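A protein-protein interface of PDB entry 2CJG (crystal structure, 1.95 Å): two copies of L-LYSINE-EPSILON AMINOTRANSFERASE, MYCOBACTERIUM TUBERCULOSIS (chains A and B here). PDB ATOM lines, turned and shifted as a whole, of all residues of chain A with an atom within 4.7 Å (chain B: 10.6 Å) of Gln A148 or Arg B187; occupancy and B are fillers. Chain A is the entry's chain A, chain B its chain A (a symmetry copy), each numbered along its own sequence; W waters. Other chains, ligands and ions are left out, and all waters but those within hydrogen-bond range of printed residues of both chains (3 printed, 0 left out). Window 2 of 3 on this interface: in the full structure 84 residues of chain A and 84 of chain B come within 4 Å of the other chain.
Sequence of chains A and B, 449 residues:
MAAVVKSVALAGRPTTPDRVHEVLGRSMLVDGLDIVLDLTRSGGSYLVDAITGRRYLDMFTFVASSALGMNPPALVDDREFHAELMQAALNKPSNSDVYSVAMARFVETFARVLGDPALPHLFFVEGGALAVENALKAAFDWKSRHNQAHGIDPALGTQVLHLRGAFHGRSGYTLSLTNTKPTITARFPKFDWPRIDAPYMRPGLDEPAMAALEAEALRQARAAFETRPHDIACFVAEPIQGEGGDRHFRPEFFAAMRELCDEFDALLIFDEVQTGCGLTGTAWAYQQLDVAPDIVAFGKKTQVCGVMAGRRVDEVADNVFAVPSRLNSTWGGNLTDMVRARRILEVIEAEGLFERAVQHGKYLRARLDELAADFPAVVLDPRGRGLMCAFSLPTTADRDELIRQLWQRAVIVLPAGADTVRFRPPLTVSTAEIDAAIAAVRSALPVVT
The guanidinium group (NE) of Arg A145 is in salt-bridge range of the side-chain carboxylate (OD1) of Asp A141. NZ of Lys B190 sits at hydrogen-bond distance from O of Phe B188 (2.7 Å). The side-chain carboxylate (OD1) of Asp A141 is in salt-bridge range of the guanidinium group (NH2) of Arg A326 (2.8 Å). OG of Ser A144 lies within hydrogen-bond range of O of Pro A154, 2.5 Å away.
The side-chain amide oxygen of Gln A148 lies within hydrogen-bond range of the guanidinium group of Arg B187, 2.9 Å away. The side-chain hydroxyl (OG) of Ser A144 lies within hydrogen-bond range of the guanidinium group (NH1) of Arg B187 (3.0 Å). NH2 of Arg A326 is in hydrogen-bond range of O of Ala B186. The guanidinium group of Arg A326 lies within hydrogen-bond range of the backbone carbonyl oxygen of Thr B183 (2.7 Å).
Of the 12 printed residues of chain B, 5 touch a printed residue of chain A. Printed residues of chain B that touch a printed residue of chain A: Thr B183, Ala B186, Arg B187, Phe B188 and Pro B189. Hydrophobic or aromatic side chains of chain B that line the printed part of chain A: Ala B186, Phe B188 and Pro B189. Printed residues of chain A that touch a printed residue of chain B: Phe A140, Asp A141, Ser A144, Arg A145, Gln A148, Pro A154 and Arg A326. Among the printed residues, no Asp or Glu carboxylate lies within 4 Å of a Lys or Arg side-chain nitrogen of the other chain.
Printed residues of chain B within 4 Å of Gln A148: Arg B187. Arg B187 touches seven residues of chain A. Of chain B, only Arg B187 (3.7 Å) comes within 4 Å of Asp A141. Of chain B, only Arg B187 (3.0 Å) comes within 4 Å of Ser A144. No residue of chain B comes within 4 Å of Ala A149. No residue of chain B comes within 4 Å of Gly A151. Of the printed residues of chain A, Pro B189 touches Phe A140. Printed residues of chain A within 4 Å of Thr B183: Arg A326. Of the printed residues of chain A, Phe B188 touches Arg A326 (3.4 Å). Of the printed residues of chain B, Arg A326 touches Thr B183, Ala B186, Arg B187 and Phe B188. Of the printed residues of chain B, Phe A140 touches Arg B187 and Pro B189. The nearest residue of chain B that does not touch Gln A148 is Ala B186 (9.1 Å).
Arg B187 touches Phe A140. Phe A140 touches Pro B189. OD1 of Asp A141 touches CD of Arg B187 (3.7 Å). Arg B187 touches Arg A145. Pro A154 touches Arg B187 (CB to NH1, 3.8 Å). NH2 of Arg A326 touches CB of Arg B187, at 3.9 Å. Phe B188 touches Arg A326 (CZ to NH2, 3.4 Å).
No position is printed for both chains.
Water W1 bridges O of Arg B187 (2.7 Å) and O of Phe A140 (3.3 Å). Water W3 lies within hydrogen-bond range of O of Arg A326 (2.7 Å) and O of Ile B184 (2.7 Å). Water W2 bridges the side-chain amide nitrogen (NE2) of Gln A148 (3.2 Å) and the guanidinium group (NH2) of Arg B187 (3.4 Å).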
ATOM      1  N   PHE A 140      23.240  10.932 -27.433  1.00  0.00           N
ATOM      2  CA  PHE A 140      23.371  12.144 -26.624  1.00  0.00           C
ATOM      3  C   PHE A 140      24.523  11.971 -25.631  1.00  0.00           C
ATOM      4  O   PHE A 140      25.341  12.870 -25.476  1.00  0.00           O
ATOM      5  CB  PHE A 140      22.103  12.441 -25.810  1.00  0.00           C
ATOM      6  CG  PHE A 140      20.885  12.758 -26.645  1.00  0.00           C
ATOM      7  CD1 PHE A 140      20.980  13.584 -27.757  1.00  0.00           C
ATOM      8  CD2 PHE A 140      19.626  12.259 -26.286  1.00  0.00           C
ATOM      9  CE1 PHE A 140      19.861  13.894 -28.502  1.00  0.00           C
ATOM     10  CE2 PHE A 140      18.496  12.553 -27.053  1.00  0.00           C
ATOM     11  CZ  PHE A 140      18.611  13.369 -28.167  1.00  0.00           C
ATOM     12  N   ASP A 141      24.564  10.836 -24.937  1.00  0.00           N
ATOM     13  CA  ASP A 141      25.628  10.582 -23.980  1.00  0.00           C
ATOM     14  C   ASP A 141      27.012  10.537 -24.667  1.00  0.00           C
ATOM     15  O   ASP A 141      27.990  11.105 -24.172  1.00  0.00           O
ATOM     16  CB  ASP A 141      25.348   9.261 -23.277  1.00  0.00           C
ATOM     17  CG  ASP A 141      26.492   8.834 -22.374  1.00  0.00           C
ATOM     18  OD1 ASP A 141      26.512   9.284 -21.207  1.00  0.00           O
ATOM     19  OD2 ASP A 141      27.320   8.022 -22.833  1.00  0.00           O
ATOM     20  N   SER A 144      28.219  14.135 -25.852  1.00  0.00           N
ATOM     21  CA  SER A 144      28.586  14.956 -24.693  1.00  0.00           C
ATOM     22  C   SER A 144      29.971  14.548 -24.158  1.00  0.00           C
ATOM     23  O   SER A 144      30.837  15.395 -23.927  1.00  0.00           O
ATOM     24  CB  SER A 144      27.535  14.760 -23.605  1.00  0.00           C
ATOM     25  OG  SER A 144      27.851  15.531 -22.469  1.00  0.00           O
ATOM     26  N   ARG A 145      30.179  13.240 -24.001  1.00  0.00           N
ATOM     27  CA  ARG A 145      31.447  12.697 -23.504  1.00  0.00           C
ATOM     28  C   ARG A 145      32.589  12.820 -24.507  1.00  0.00           C
ATOM     29  O   ARG A 145      33.726  13.104 -24.102  1.00  0.00           O
ATOM     30  CB  ARG A 145      31.285  11.248 -23.091  1.00  0.00           C
ATOM     31  CG  ARG A 145      30.367  11.089 -21.903  1.00  0.00           C
ATOM     32  CD  ARG A 145      30.302   9.608 -21.505  1.00  0.00           C
ATOM     33  NE  ARG A 145      29.270   9.329 -20.509  1.00  0.00           N
ATOM     34  CZ  ARG A 145      29.467   9.388 -19.196  1.00  0.00           C
ATOM     35  NH1 ARG A 145      28.485   9.066 -18.373  1.00  0.00           N
ATOM     36  NH2 ARG A 145      30.655   9.735 -18.694  1.00  0.00           N
ATOM     37  N   HIS A 146      32.283  12.645 -25.795  1.00  0.00           N
ATOM     38  CA  HIS A 146      33.274  12.837 -26.858  1.00  0.00           C
ATOM     39  C   HIS A 146      33.702  14.322 -26.859  1.00  0.00           C
ATOM     40  O   HIS A 146      34.895  14.624 -26.814  1.00  0.00           O
ATOM     41  CB  HIS A 146      32.702  12.411 -28.207  1.00  0.00           C
ATOM     42  CG  HIS A 146      33.697  12.412 -29.327  1.00  0.00           C
ATOM     43  ND1 HIS A 146      33.879  13.497 -30.162  1.00  0.00           N
ATOM     44  CD2 HIS A 146      34.526  11.442 -29.783  1.00  0.00           C
ATOM     45  CE1 HIS A 146      34.791  13.204 -31.069  1.00  0.00           C
ATOM     46  NE2 HIS A 146      35.211  11.969 -30.852  1.00  0.00           N
ATOM     47  N   ASN A 147      32.728  15.227 -26.869  1.00  0.00           N
ATOM     48  CA  ASN A 147      32.966  16.661 -26.698  1.00  0.00           C
ATOM     49  C   ASN A 147      33.888  16.958 -25.514  1.00  0.00           C
ATOM     50  O   ASN A 147      34.941  17.576 -25.679  1.00  0.00           O
ATOM     51  CB  ASN A 147      31.642  17.400 -26.509  1.00  0.00           C
ATOM     52  CG  ASN A 147      30.938  17.721 -27.839  1.00  0.00           C
ATOM     53  OD1 ASN A 147      31.514  17.610 -28.931  1.00  0.00           O
ATOM     54  ND2 ASN A 147      29.692  18.162 -27.734  1.00  0.00           N
ATOM     55  N   GLN A 148      33.486  16.498 -24.331  1.00  0.00           N
ATOM     56  CA  GLN A 148      34.243  16.696 -23.095  1.00  0.00           C
ATOM     57  C   GLN A 148      35.697  16.232 -23.241  1.00  0.00           C
ATOM     58  O   GLN A 148      36.604  16.899 -22.744  1.00  0.00           O
ATOM     59  CB  GLN A 148      33.559  15.945 -21.956  1.00  0.00           C
ATOM     60  CG  GLN A 148      34.203  16.092 -20.587  1.00  0.00           C
ATOM     61  CD  GLN A 148      33.369  15.468 -19.475  1.00  0.00           C
ATOM     62  OE1 GLN A 148      32.138  15.342 -19.571  1.00  0.00           O
ATOM     63  NE2 GLN A 148      34.044  15.060 -18.405  1.00  0.00           N
ATOM     64  N   ALA A 149      35.907  15.106 -23.931  1.00  0.00           N
ATOM     65  CA  ALA A 149      37.231  14.510 -24.065  1.00  0.00           C
ATOM     66  C   ALA A 149      38.129  15.344 -24.962  1.00  0.00           C
ATOM     67  O   ALA A 149      39.340  15.275 -24.838  1.00  0.00           O
ATOM     68  CB  ALA A 149      37.140  13.068 -24.592  1.00  0.00           C
ATOM     69  N   HIS A 150      37.534  16.127 -25.856  1.00  0.00           N
ATOM     70  CA  HIS A 150      38.281  16.992 -26.771  1.00  0.00           C
ATOM     71  C   HIS A 150      38.157  18.471 -26.407  1.00  0.00           C
ATOM     72  O   HIS A 150      38.307  19.352 -27.242  1.00  0.00           O
ATOM     73  CB  HIS A 150      37.828  16.745 -28.212  1.00  0.00           C
ATOM     74  CG  HIS A 150      37.996  15.327 -28.648  1.00  0.00           C
ATOM     75  ND1 HIS A 150      38.968  14.934 -29.541  1.00  0.00           N
ATOM     76  CD2 HIS A 150      37.346  14.196 -28.282  1.00  0.00           C
ATOM     77  CE1 HIS A 150      38.898  13.627 -29.725  1.00  0.00           C
ATOM     78  NE2 HIS A 150      37.927  13.155 -28.963  1.00  0.00           N
ATOM     79  N   GLY A 151      37.888  18.741 -25.145  1.00  0.00           N
ATOM     80  CA  GLY A 151      37.876  20.109 -24.664  1.00  0.00           C
ATOM     81  C   GLY A 151      36.681  20.951 -25.044  1.00  0.00           C
ATOM     82  O   GLY A 151      36.696  22.159 -24.821  1.00  0.00           O
ATOM     83  N   ILE A 152      35.645  20.326 -25.611  1.00  0.00           N
ATOM     84  CA  ILE A 152      34.394  21.009 -25.936  1.00  0.00           C
ATOM     85  C   ILE A 152      33.398  20.893 -24.771  1.00  0.00           C
ATOM     86  O   ILE A 152      33.378  19.885 -24.048  1.00  0.00           O
ATOM     87  CB  ILE A 152      33.817  20.453 -27.246  1.00  0.00           C
ATOM     88  CG1 ILE A 152      34.845  20.642 -28.362  1.00  0.00           C
ATOM     89  CG2 ILE A 152      32.517  21.128 -27.603  1.00  0.00           C
ATOM     90  CD1 ILE A 152      34.658  19.765 -29.557  1.00  0.00           C
ATOM     91  N   PRO A 154      30.609  19.928 -22.483  1.00  0.00           N
ATOM     92  CA  PRO A 154      29.773  18.713 -22.483  1.00  0.00           C
ATOM     93  C   PRO A 154      28.264  18.984 -22.425  1.00  0.00           C
ATOM     94  O   PRO A 154      27.462  18.036 -22.480  1.00  0.00           O
ATOM     95  CB  PRO A 154      30.252  17.959 -21.236  1.00  0.00           C
ATOM     96  CG  PRO A 154      30.702  19.041 -20.306  1.00  0.00           C
ATOM     97  CD  PRO A 154      31.336  20.080 -21.204  1.00  0.00           C
ATOM     98  N   ARG A 326      22.580   3.687 -16.804  1.00  0.00           N
ATOM     99  CA  ARG A 326      22.327   4.824 -17.703  1.00  0.00           C
ATOM    100  C   ARG A 326      21.071   4.601 -18.566  1.00  0.00           C
ATOM    101  O   ARG A 326      20.340   5.540 -18.866  1.00  0.00           O
ATOM    102  CB  ARG A 326      23.553   5.092 -18.598  1.00  0.00           C
ATOM    103  CG  ARG A 326      24.796   5.542 -17.823  1.00  0.00           C
ATOM    104  CD  ARG A 326      24.621   6.963 -17.352  1.00  0.00           C
ATOM    105  NE  ARG A 326      24.732   7.882 -18.478  1.00  0.00           N
ATOM    106  CZ  ARG A 326      24.072   9.034 -18.595  1.00  0.00           C
ATOM    107  NH1 ARG A 326      23.204   9.430 -17.653  1.00  0.00           N
ATOM    108  NH2 ARG A 326      24.280   9.792 -19.659  1.00  0.00           N
ATOM    109  N   LEU B 175      12.073  12.009 -18.427  1.00  0.00           N
ATOM    110  CA  LEU B 175      13.425  12.426 -18.015  1.00  0.00           C
ATOM    111  C   LEU B 175      13.445  13.885 -17.601  1.00  0.00           C
ATOM    112  O   LEU B 175      14.365  14.322 -16.902  1.00  0.00           O
ATOM    113  CB  LEU B 175      14.408  12.218 -19.176  1.00  0.00           C
ATOM    114  CG  LEU B 175      15.403  11.040 -19.308  1.00  0.00           C
ATOM    115  CD1 LEU B 175      15.582  10.036 -18.152  1.00  0.00           C
ATOM    116  CD2 LEU B 175      15.403  10.408 -20.722  1.00  0.00           C
ATOM    117  N   SER B 176      12.426  14.641 -18.021  1.00  0.00           N
ATOM    118  CA  SER B 176      12.286  16.056 -17.614  1.00  0.00           C
ATOM    119  C   SER B 176      11.589  16.178 -16.257  1.00  0.00           C
ATOM    120  O   SER B 176      11.547  17.279 -15.666  1.00  0.00           O
ATOM    121  CB  SER B 176      11.565  16.888 -18.671  1.00  0.00           C
ATOM    122  OG  SER B 176      12.335  16.975 -19.868  1.00  0.00           O
ATOM    123  N   LYS B 181      18.580  10.155  -8.687  1.00  0.00           N
ATOM    124  CA  LYS B 181      20.010  10.125  -8.937  1.00  0.00           C
ATOM    125  C   LYS B 181      20.366  10.799 -10.267  1.00  0.00           C
ATOM    126  O   LYS B 181      19.719  10.535 -11.301  1.00  0.00           O
ATOM    127  CB  LYS B 181      20.473   8.681  -9.045  1.00  0.00           C
ATOM    128  CG  LYS B 181      20.593   7.956  -7.754  1.00  0.00           C
ATOM    129  CD  LYS B 181      21.224   6.603  -8.048  1.00  0.00           C
ATOM    130  CE  LYS B 181      20.279   5.472  -7.690  1.00  0.00           C
ATOM    131  NZ  LYS B 181      20.334   5.292  -6.198  1.00  0.00           N
ATOM    132  N   PRO B 182      21.439  11.609 -10.267  1.00  0.00           N
ATOM    133  CA  PRO B 182      21.988  12.279 -11.458  1.00  0.00           C
ATOM    134  C   PRO B 182      22.306  11.330 -12.615  1.00  0.00           C
ATOM    135  O   PRO B 182      22.154  11.715 -13.767  1.00  0.00           O
ATOM    136  CB  PRO B 182      23.278  12.922 -10.927  1.00  0.00           C
ATOM    137  CG  PRO B 182      22.981  13.190  -9.472  1.00  0.00           C
ATOM    138  CD  PRO B 182      22.200  11.953  -9.051  1.00  0.00           C
ATOM    139  N   THR B 183      22.751  10.107 -12.295  1.00  0.00           N
ATOM    140  CA  THR B 183      23.026   9.037 -13.271  1.00  0.00           C
ATOM    141  C   THR B 183      21.852   8.792 -14.231  1.00  0.00           C
ATOM    142  O   THR B 183      22.049   8.432 -15.405  1.00  0.00           O
ATOM    143  CB  THR B 183      23.337   7.705 -12.507  1.00  0.00           C
ATOM    144  OG1 THR B 183      24.583   7.855 -11.831  1.00  0.00           O
ATOM    145  CG2 THR B 183      23.421   6.460 -13.434  1.00  0.00           C
ATOM    146  N   ILE B 184      20.635   8.974 -13.732  1.00  0.00           N
ATOM    147  CA  ILE B 184      19.455   8.667 -14.537  1.00  0.00           C
ATOM    148  C   ILE B 184      19.230   9.673 -15.671  1.00  0.00           C
ATOM    149  O   ILE B 184      18.796   9.289 -16.757  1.00  0.00           O
ATOM    150  CB  ILE B 184      18.193   8.505 -13.657  1.00  0.00           C
ATOM    151  CG1 ILE B 184      18.405   7.303 -12.727  1.00  0.00           C
ATOM    152  CG2 ILE B 184      16.926   8.297 -14.525  1.00  0.00           C
ATOM    153  CD1 ILE B 184      17.380   7.214 -11.590  1.00  0.00           C
ATOM    154  N   THR B 185      19.569  10.934 -15.419  1.00  0.00           N
ATOM    155  CA  THR B 185      19.173  12.025 -16.288  1.00  0.00           C
ATOM    156  C   THR B 185      20.331  12.796 -16.916  1.00  0.00           C
ATOM    157  O   THR B 185      20.103  13.538 -17.850  1.00  0.00           O
ATOM    158  CB  THR B 185      18.247  13.022 -15.543  1.00  0.00           C
ATOM    159  OG1 THR B 185      18.873  13.396 -14.321  1.00  0.00           O
ATOM    160  CG2 THR B 185      16.917  12.362 -15.207  1.00  0.00           C
ATOM    161  N   ALA B 186      21.570  12.601 -16.434  1.00  0.00           N
ATOM    162  CA  ALA B 186      22.709  13.406 -16.921  1.00  0.00           C
ATOM    163  C   ALA B 186      22.925  13.287 -18.425  1.00  0.00           C
ATOM    164  O   ALA B 186      22.827  12.187 -18.990  1.00  0.00           O
ATOM    165  CB  ALA B 186      24.004  13.040 -16.159  1.00  0.00           C
ATOM    166  N   ARG B 187      23.176  14.430 -19.072  1.00  0.00           N
ATOM    167  CA  ARG B 187      23.558  14.481 -20.486  1.00  0.00           C
ATOM    168  C   ARG B 187      22.399  14.186 -21.447  1.00  0.00           C
ATOM    169  O   ARG B 187      22.605  14.054 -22.670  1.00  0.00           O
ATOM    170  CB  ARG B 187      24.751  13.540 -20.794  1.00  0.00           C
ATOM    171  CG  ARG B 187      25.902  13.613 -19.766  1.00  0.00           C
ATOM    172  CD  ARG B 187      27.122  12.841 -20.251  1.00  0.00           C
ATOM    173  NE  ARG B 187      28.199  12.862 -19.254  1.00  0.00           N
ATOM    174  CZ  ARG B 187      29.343  13.556 -19.367  1.00  0.00           C
ATOM    175  NH1 ARG B 187      29.626  14.286 -20.449  1.00  0.00           N
ATOM    176  NH2 ARG B 187      30.235  13.466 -18.393  1.00  0.00           N
ATOM    177  N   PHE B 188      21.179  14.104 -20.918  1.00  0.00           N
ATOM    178  CA  PHE B 188      19.986  13.938 -21.787  1.00  0.00           C
ATOM    179  C   PHE B 188      19.206  15.260 -21.884  1.00  0.00           C
ATOM    180  O   PHE B 188      18.993  15.918 -20.864  1.00  0.00           O
ATOM    181  CB  PHE B 188      19.105  12.811 -21.263  1.00  0.00           C
ATOM    182  CG  PHE B 188      19.828  11.487 -21.108  1.00  0.00           C
ATOM    183  CD1 PHE B 188      20.635  10.969 -22.159  1.00  0.00           C
ATOM    184  CD2 PHE B 188      19.712  10.757 -19.923  1.00  0.00           C
ATOM    185  CE1 PHE B 188      21.307   9.760 -22.000  1.00  0.00           C
ATOM    186  CE2 PHE B 188      20.372   9.539 -19.755  1.00  0.00           C
ATOM    187  CZ  PHE B 188      21.170   9.035 -20.803  1.00  0.00           C
ATOM    188  N   PRO B 189      18.811  15.673 -23.099  1.00  0.00           N
ATOM    189  CA  PRO B 189      18.022  16.915 -23.190  1.00  0.00           C
ATOM    190  C   PRO B 189      16.667  16.895 -22.440  1.00  0.00           C
ATOM    191  O   PRO B 189      15.960  15.867 -22.400  1.00  0.00           O
ATOM    192  CB  PRO B 189      17.822  17.129 -24.704  1.00  0.00           C
ATOM    193  CG  PRO B 189      18.173  15.797 -25.362  1.00  0.00           C
ATOM    194  CD  PRO B 189      19.110  15.083 -24.425  1.00  0.00           C
ATOM    195  N   LYS B 190      16.326  18.049 -21.872  1.00  0.00           N
ATOM    196  CA  LYS B 190      15.161  18.180 -21.004  1.00  0.00           C
ATOM    197  C   LYS B 190      14.427  19.472 -21.302  1.00  0.00           C
ATOM    198  O   LYS B 190      15.019  20.432 -21.805  1.00  0.00           O
ATOM    199  CB  LYS B 190      15.584  18.148 -19.530  1.00  0.00           C
ATOM    200  CG  LYS B 190      16.237  16.831 -19.107  1.00  0.00           C
ATOM    201  CD  LYS B 190      16.643  16.810 -17.641  1.00  0.00           C
ATOM    202  CE  LYS B 190      18.124  17.090 -17.441  1.00  0.00           C
ATOM    203  NZ  LYS B 190      19.052  16.133 -18.164  1.00  0.00           N
HETATM  204  O   HOH W   1      23.889  15.593 -24.436  1.00  0.00           O
HETATM  205  O   HOH W   2      32.434  14.087 -15.841  1.00  0.00           O
HETATM  206  O   HOH W   3      18.179   6.958 -18.025  1.00  0.00           O
